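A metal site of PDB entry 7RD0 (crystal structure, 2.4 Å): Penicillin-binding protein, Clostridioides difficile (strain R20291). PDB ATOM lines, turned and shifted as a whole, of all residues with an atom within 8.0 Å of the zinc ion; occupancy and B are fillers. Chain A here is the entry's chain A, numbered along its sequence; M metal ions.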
ATOM      1  N   TYR A 280     -12.680  -5.496 -12.880  1.00  0.00           N
ATOM      2  CA  TYR A 280     -12.728  -6.540 -13.938  1.00  0.00           C
ATOM      3  C   TYR A 280     -11.325  -6.795 -14.495  1.00  0.00           C
ATOM      4  O   TYR A 280     -10.547  -5.817 -14.746  1.00  0.00           O
ATOM      5  CB  TYR A 280     -13.700  -6.170 -15.059  1.00  0.00           C
ATOM      6  CG  TYR A 280     -13.789  -7.209 -16.145  1.00  0.00           C
ATOM      7  CD1 TYR A 280     -14.662  -8.288 -16.016  1.00  0.00           C
ATOM      8  CD2 TYR A 280     -12.984  -7.147 -17.280  1.00  0.00           C
ATOM      9  CE1 TYR A 280     -14.732  -9.282 -16.992  1.00  0.00           C
ATOM     10  CE2 TYR A 280     -13.064  -8.121 -18.262  1.00  0.00           C
ATOM     11  CZ  TYR A 280     -13.931  -9.194 -18.110  1.00  0.00           C
ATOM     12  OH  TYR A 280     -14.024 -10.174 -19.062  1.00  0.00           O
ATOM     13  N   ASN A 281     -10.998  -8.088 -14.690  1.00  0.00           N
ATOM     14  CA  ASN A 281      -9.701  -8.561 -15.218  1.00  0.00           C
ATOM     15  C   ASN A 281      -9.885  -8.855 -16.709  1.00  0.00           C
ATOM     16  O   ASN A 281     -10.440  -9.913 -17.079  1.00  0.00           O
ATOM     17  CB  ASN A 281      -9.151  -9.776 -14.481  1.00  0.00           C
ATOM     18  CG  ASN A 281      -7.756 -10.188 -14.931  1.00  0.00           C
ATOM     19  OD1 ASN A 281      -7.098  -9.486 -15.701  1.00  0.00           O
ATOM     20  ND2 ASN A 281      -7.305 -11.339 -14.457  1.00  0.00           N
ATOM     21  N   CYS A 282      -9.411  -7.923 -17.527  1.00  0.00           N
ATOM     22  CA  CYS A 282      -9.439  -8.085 -18.986  1.00  0.00           C
ATOM     23  C   CYS A 282      -8.178  -8.850 -19.401  1.00  0.00           C
ATOM     24  O   CYS A 282      -7.071  -8.274 -19.259  1.00  0.00           O
ATOM     25  CB  CYS A 282      -9.523  -6.724 -19.653  1.00  0.00           C
ATOM     26  SG  CYS A 282      -9.418  -6.835 -21.446  1.00  0.00           S
ATOM     27  N   THR A 283      -8.359 -10.082 -19.862  1.00  0.00           N
ATOM     28  CA  THR A 283      -7.296 -10.963 -20.417  1.00  0.00           C
ATOM     29  C   THR A 283      -7.209 -10.798 -21.931  1.00  0.00           C
ATOM     30  O   THR A 283      -6.323 -11.431 -22.543  1.00  0.00           O
ATOM     31  CB  THR A 283      -7.544 -12.429 -20.072  1.00  0.00           C
ATOM     32  OG1 THR A 283      -8.794 -12.838 -20.625  1.00  0.00           O
ATOM     33  CG2 THR A 283      -7.513 -12.660 -18.580  1.00  0.00           C
ATOM     34  N   GLY A 284      -8.091  -9.977 -22.505  1.00  0.00           N
ATOM     35  CA  GLY A 284      -8.093  -9.658 -23.950  1.00  0.00           C
ATOM     36  C   GLY A 284      -9.227 -10.332 -24.698  1.00  0.00           C
ATOM     37  O   GLY A 284      -9.451  -9.998 -25.870  1.00  0.00           O
ATOM     38  N   LYS A 285      -9.921 -11.271 -24.055  1.00  0.00           N
ATOM     39  CA  LYS A 285     -11.089 -11.966 -24.652  1.00  0.00           C
ATOM     40  C   LYS A 285     -11.998 -12.479 -23.551  1.00  0.00           C
ATOM     41  O   LYS A 285     -11.544 -12.575 -22.402  1.00  0.00           O
ATOM     42  CB  LYS A 285     -10.640 -13.120 -25.565  1.00  0.00           C
ATOM     43  CG  LYS A 285      -9.789 -14.213 -24.917  1.00  0.00           C
ATOM     44  CD  LYS A 285      -9.625 -15.412 -25.847  1.00  0.00           C
ATOM     45  CE  LYS A 285      -8.216 -15.966 -25.892  1.00  0.00           C
ATOM     46  NZ  LYS A 285      -7.951 -16.836 -24.728  1.00  0.00           N
ATOM     47  N   ARG A 296     -13.420 -10.439 -28.335  1.00  0.00           N
ATOM     48  CA  ARG A 296     -12.067  -9.957 -28.004  1.00  0.00           C
ATOM     49  C   ARG A 296     -12.136  -8.491 -27.593  1.00  0.00           C
ATOM     50  O   ARG A 296     -13.051  -7.790 -28.005  1.00  0.00           O
ATOM     51  CB  ARG A 296     -11.162 -10.056 -29.235  1.00  0.00           C
ATOM     52  CG  ARG A 296     -11.269 -11.385 -29.969  1.00  0.00           C
ATOM     53  CD  ARG A 296      -9.953 -11.772 -30.623  1.00  0.00           C
ATOM     54  NE  ARG A 296      -9.704 -13.203 -30.525  1.00  0.00           N
ATOM     55  CZ  ARG A 296      -8.707 -13.754 -29.842  1.00  0.00           C
ATOM     56  NH1 ARG A 296      -7.849 -12.988 -29.202  1.00  0.00           N
ATOM     57  NH2 ARG A 296      -8.573 -15.064 -29.825  1.00  0.00           N
ATOM     58  N   CYS A 297     -11.188  -8.095 -26.762  1.00  0.00           N
ATOM     59  CA  CYS A 297     -10.929  -6.671 -26.387  1.00  0.00           C
ATOM     60  C   CYS A 297     -10.133  -6.041 -27.525  1.00  0.00           C
ATOM     61  O   CYS A 297      -9.538  -6.795 -28.322  1.00  0.00           O
ATOM     62  CB  CYS A 297     -10.175  -6.569 -25.059  1.00  0.00           C
ATOM     63  SG  CYS A 297      -9.954  -4.865 -24.461  1.00  0.00           S
ATOM     64  N   ASN A 298     -10.122  -4.708 -27.606  1.00  0.00           N
ATOM     65  CA  ASN A 298      -9.324  -3.963 -28.622  1.00  0.00           C
ATOM     66  C   ASN A 298      -7.845  -4.065 -28.285  1.00  0.00           C
ATOM     67  O   ASN A 298      -7.052  -3.986 -29.222  1.00  0.00           O
ATOM     68  CB  ASN A 298      -9.780  -2.499 -28.777  1.00  0.00           C
ATOM     69  CG  ASN A 298     -11.147  -2.398 -29.431  1.00  0.00           C
ATOM     70  OD1 ASN A 298     -11.515  -3.242 -30.233  1.00  0.00           O
ATOM     71  ND2 ASN A 298     -11.908  -1.369 -29.078  1.00  0.00           N
ATOM     72  N   LYS A 299      -7.494  -4.267 -27.001  1.00  0.00           N
ATOM     73  CA  LYS A 299      -6.076  -4.433 -26.583  1.00  0.00           C
ATOM     74  C   LYS A 299      -5.577  -5.816 -27.014  1.00  0.00           C
ATOM     75  O   LYS A 299      -4.430  -5.898 -27.511  1.00  0.00           O
ATOM     76  CB  LYS A 299      -5.899  -4.108 -25.088  1.00  0.00           C
ATOM     77  CG  LYS A 299      -4.483  -3.737 -24.677  1.00  0.00           C
ATOM     78  CD  LYS A 299      -4.368  -2.514 -23.768  1.00  0.00           C
ATOM     79  CE  LYS A 299      -2.993  -2.325 -23.146  1.00  0.00           C
ATOM     80  NZ  LYS A 299      -1.900  -2.908 -23.977  1.00  0.00           N
ATOM     81  N   ARG A 300      -6.402  -6.865 -26.900  1.00  0.00           N
ATOM     82  CA  ARG A 300      -6.148  -8.232 -27.448  1.00  0.00           C
ATOM     83  C   ARG A 300      -5.316  -9.046 -26.445  1.00  0.00           C
ATOM     84  O   ARG A 300      -5.735 -10.177 -26.130  1.00  0.00           O
ATOM     85  CB  ARG A 300      -5.492  -8.229 -28.834  1.00  0.00           C
ATOM     86  CG  ARG A 300      -5.251  -9.620 -29.395  1.00  0.00           C
ATOM     87  CD  ARG A 300      -4.965  -9.686 -30.895  1.00  0.00           C
ATOM     88  NE  ARG A 300      -6.135  -9.980 -31.711  1.00  0.00           N
ATOM     89  CZ  ARG A 300      -6.591 -11.206 -32.020  1.00  0.00           C
ATOM     90  NH1 ARG A 300      -5.978 -12.286 -31.560  1.00  0.00           N
ATOM     91  NH2 ARG A 300      -7.663 -11.344 -32.787  1.00  0.00           N
ATOM     92  N   ASP A 301      -4.203  -8.487 -25.952  1.00  0.00           N
ATOM     93  CA  ASP A 301      -3.381  -9.048 -24.831  1.00  0.00           C
ATOM     94  C   ASP A 301      -3.909  -8.573 -23.474  1.00  0.00           C
ATOM     95  O   ASP A 301      -3.344  -8.999 -22.457  1.00  0.00           O
ATOM     96  CB  ASP A 301      -1.901  -8.653 -24.962  1.00  0.00           C
ATOM     97  CG  ASP A 301      -1.647  -7.157 -25.009  1.00  0.00           C
ATOM     98  OD1 ASP A 301      -2.579  -6.387 -25.380  1.00  0.00           O
ATOM     99  OD2 ASP A 301      -0.519  -6.745 -24.683  1.00  0.00           O
ATOM    100  N   GLY A 302      -4.905  -7.671 -23.447  1.00  0.00           N
ATOM    101  CA  GLY A 302      -5.723  -7.348 -22.255  1.00  0.00           C
ATOM    102  C   GLY A 302      -5.314  -6.060 -21.560  1.00  0.00           C
ATOM    103  O   GLY A 302      -4.134  -5.659 -21.649  1.00  0.00           O
ATOM    104  N   HIS A 303      -6.283  -5.416 -20.898  1.00  0.00           N
ATOM    105  CA  HIS A 303      -6.093  -4.204 -20.045  1.00  0.00           C
ATOM    106  C   HIS A 303      -5.597  -4.652 -18.666  1.00  0.00           C
ATOM    107  O   HIS A 303      -5.077  -3.800 -17.935  1.00  0.00           O
ATOM    108  CB  HIS A 303      -7.403  -3.382 -19.934  1.00  0.00           C
ATOM    109  CG  HIS A 303      -7.832  -2.761 -21.228  1.00  0.00           C
ATOM    110  ND1 HIS A 303      -8.834  -3.318 -21.991  1.00  0.00           N
ATOM    111  CD2 HIS A 303      -7.336  -1.724 -21.931  1.00  0.00           C
ATOM    112  CE1 HIS A 303      -8.961  -2.616 -23.109  1.00  0.00           C
ATOM    113  NE2 HIS A 303      -8.043  -1.625 -23.093  1.00  0.00           N
ATOM    114  N   GLY A 304      -5.774  -5.923 -18.306  1.00  0.00           N
ATOM    115  CA  GLY A 304      -5.481  -6.441 -16.959  1.00  0.00           C
ATOM    116  C   GLY A 304      -6.532  -5.986 -15.975  1.00  0.00           C
ATOM    117  O   GLY A 304      -7.652  -5.673 -16.405  1.00  0.00           O
ATOM    118  N   GLN A 306      -8.787  -3.820 -13.810  1.00  0.00           N
ATOM    119  CA  GLN A 306      -9.312  -2.458 -14.055  1.00  0.00           C
ATOM    120  C   GLN A 306     -10.321  -2.167 -12.944  1.00  0.00           C
ATOM    121  O   GLN A 306     -11.115  -3.076 -12.621  1.00  0.00           O
ATOM    122  CB  GLN A 306     -10.009  -2.389 -15.411  1.00  0.00           C
ATOM    123  CG  GLN A 306      -9.082  -2.418 -16.615  1.00  0.00           C
ATOM    124  CD  GLN A 306      -9.883  -2.632 -17.874  1.00  0.00           C
ATOM    125  OE1 GLN A 306     -10.044  -1.720 -18.687  1.00  0.00           O
ATOM    126  NE2 GLN A 306     -10.425  -3.836 -18.023  1.00  0.00           N
ATOM    127  N   GLN A 310     -11.174   2.822 -14.984  1.00  0.00           N
ATOM    128  CA  GLN A 310     -10.236   2.354 -16.035  1.00  0.00           C
ATOM    129  C   GLN A 310     -11.000   1.572 -17.092  1.00  0.00           C
ATOM    130  O   GLN A 310     -10.737   1.791 -18.309  1.00  0.00           O
ATOM    131  CB  GLN A 310      -9.080   1.554 -15.428  1.00  0.00           C
ATOM    132  CG  GLN A 310      -8.117   2.403 -14.613  1.00  0.00           C
ATOM    133  CD  GLN A 310      -7.289   1.580 -13.650  1.00  0.00           C
ATOM    134  OE1 GLN A 310      -7.768   0.615 -13.040  1.00  0.00           O
ATOM    135  NE2 GLN A 310      -6.038   1.971 -13.527  1.00  0.00           N
ATOM    136  N   ALA A 311     -11.906   0.687 -16.672  1.00  0.00           N
ATOM    137  CA  ALA A 311     -12.777  -0.098 -17.589  1.00  0.00           C
ATOM    138  C   ALA A 311     -13.499   0.865 -18.539  1.00  0.00           C
ATOM    139  O   ALA A 311     -13.434   0.665 -19.778  1.00  0.00           O
ATOM    140  CB  ALA A 311     -13.747  -0.902 -16.765  1.00  0.00           C
ATOM    141  N   ASN A 314     -10.736   2.973 -20.660  1.00  0.00           N
ATOM    142  CA  ASN A 314     -10.092   2.063 -21.647  1.00  0.00           C
ATOM    143  C   ASN A 314     -11.117   1.590 -22.688  1.00  0.00           C
ATOM    144  O   ASN A 314     -10.677   1.016 -23.744  1.00  0.00           O
ATOM    145  CB  ASN A 314      -9.449   0.848 -20.973  1.00  0.00           C
ATOM    146  CG  ASN A 314      -8.303   1.227 -20.078  1.00  0.00           C
ATOM    147  OD1 ASN A 314      -7.561   2.148 -20.402  1.00  0.00           O
ATOM    148  ND2 ASN A 314      -8.155   0.532 -18.953  1.00  0.00           N
ATOM    149  N   SER A 315     -12.407   1.780 -22.409  1.00  0.00           N
ATOM    150  CA  SER A 315     -13.475   1.399 -23.379  1.00  0.00           C
ATOM    151  C   SER A 315     -13.426  -0.133 -23.575  1.00  0.00           C
ATOM    152  O   SER A 315     -13.547  -0.607 -24.713  1.00  0.00           O
ATOM    153  CB  SER A 315     -13.264   2.208 -24.675  1.00  0.00           C
ATOM    154  OG  SER A 315     -14.396   2.204 -25.544  1.00  0.00           O
ATOM    155  N   CYS A 316     -13.269  -0.880 -22.485  1.00  0.00           N
ATOM    156  CA  CYS A 316     -12.942  -2.330 -22.506  1.00  0.00           C
ATOM    157  C   CYS A 316     -14.251  -3.124 -22.724  1.00  0.00           C
ATOM    158  O   CYS A 316     -15.098  -3.188 -21.771  1.00  0.00           O
ATOM    159  CB  CYS A 316     -12.208  -2.739 -21.226  1.00  0.00           C
ATOM    160  SG  CYS A 316     -11.934  -4.521 -21.002  1.00  0.00           S
ATOM    161  N   ASN A 317     -14.416  -3.657 -23.943  1.00  0.00           N
ATOM    162  CA  ASN A 317     -15.640  -4.376 -24.378  1.00  0.00           C
ATOM    163  C   ASN A 317     -15.923  -5.534 -23.430  1.00  0.00           C
ATOM    164  O   ASN A 317     -17.047  -5.647 -22.951  1.00  0.00           O
ATOM    165  CB  ASN A 317     -15.528  -4.827 -25.840  1.00  0.00           C
ATOM    166  CG  ASN A 317     -15.586  -3.695 -26.832  1.00  0.00           C
ATOM    167  OD1 ASN A 317     -16.240  -2.680 -26.603  1.00  0.00           O
ATOM    168  ND2 ASN A 317     -14.902  -3.852 -27.951  1.00  0.00           N
ATOM    169  N   PRO A 318     -14.954  -6.433 -23.133  1.00  0.00           N
ATOM    170  CA  PRO A 318     -15.194  -7.518 -22.168  1.00  0.00           C
ATOM    171  C   PRO A 318     -15.714  -7.042 -20.804  1.00  0.00           C
ATOM    172  O   PRO A 318     -16.578  -7.686 -20.265  1.00  0.00           O
ATOM    173  CB  PRO A 318     -13.811  -8.171 -21.984  1.00  0.00           C
ATOM    174  CG  PRO A 318     -13.126  -7.886 -23.302  1.00  0.00           C
ATOM    175  CD  PRO A 318     -13.611  -6.502 -23.722  1.00  0.00           C
ATOM    176  N   ALA A 319     -15.170  -5.955 -20.240  1.00  0.00           N
ATOM    177  CA  ALA A 319     -15.676  -5.430 -18.946  1.00  0.00           C
ATOM    178  C   ALA A 319     -17.147  -4.997 -19.104  1.00  0.00           C
ATOM    179  O   ALA A 319     -17.958  -5.268 -18.183  1.00  0.00           O
ATOM    180  CB  ALA A 319     -14.808  -4.317 -18.440  1.00  0.00           C
ATOM    181  N   PHE A 320     -17.512  -4.389 -20.241  1.00  0.00           N
ATOM    182  CA  PHE A 320     -18.885  -3.821 -20.439  1.00  0.00           C
ATOM    183  C   PHE A 320     -19.884  -4.936 -20.808  1.00  0.00           C
ATOM    184  O   PHE A 320     -21.038  -4.855 -20.318  1.00  0.00           O
ATOM    185  CB  PHE A 320     -18.863  -2.559 -21.312  1.00  0.00           C
ATOM    186  CG  PHE A 320     -18.623  -1.336 -20.456  1.00  0.00           C
ATOM    187  CD1 PHE A 320     -19.665  -0.706 -19.816  1.00  0.00           C
ATOM    188  CD2 PHE A 320     -17.333  -0.907 -20.184  1.00  0.00           C
ATOM    189  CE1 PHE A 320     -19.440   0.370 -18.969  1.00  0.00           C
ATOM    190  CE2 PHE A 320     -17.109   0.169 -19.338  1.00  0.00           C
ATOM    191  CZ  PHE A 320     -18.162   0.808 -18.730  1.00  0.00           C
HETATM  192 ZN    ZN M   1     -10.139  -4.801 -22.261  1.00  0.00          ZN
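The backbone NH (N) of Lys 299 sits close to the side-chain sulfur (SG) of Cys 297, at 3.6 Å. The backbone NH (N) of Cys 297 lies within hydrogen-bond range of the backbone carbonyl oxygen (O) of Gly 284 (2.7 Å). The side-chain sulfur (SG) of Cys 316 lies close to the side-chain amide nitrogen (NE2) of Gln 306, at 3.4 Å. The side-chain sulfur (SG) of Cys 316 lies close to the backbone NH (N) of Ala 319, at 3.6 Å. The backbone NH (N) of Cys 316 sits at hydrogen-bond distance from the backbone carbonyl oxygen (O) of Ala 311 (3.1 Å). The backbone NH (N) of Gly 284 lies close to the side-chain sulfur (SG) of Cys 282 (3.6 Å). The backbone NH (N) of Gly 304 is in hydrogen-bond range of the backbone carbonyl oxygen (O) of Cys 282 (2.8 Å).
Of the 25 residues printed, 4 come within 4 Å of the zinc ion.
The zinc ion is bound by a ring nitrogen (ND1) of His 303 (2.0 Å), the side-chain sulfur (SG) of Cys 297 (2.2 Å), the side-chain sulfur (SG) of Cys 316 (2.2 Å) and the side-chain sulfur (SG) of Cys 282 (2.3 Å). The zinc ion has four donor atoms within binding distance.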
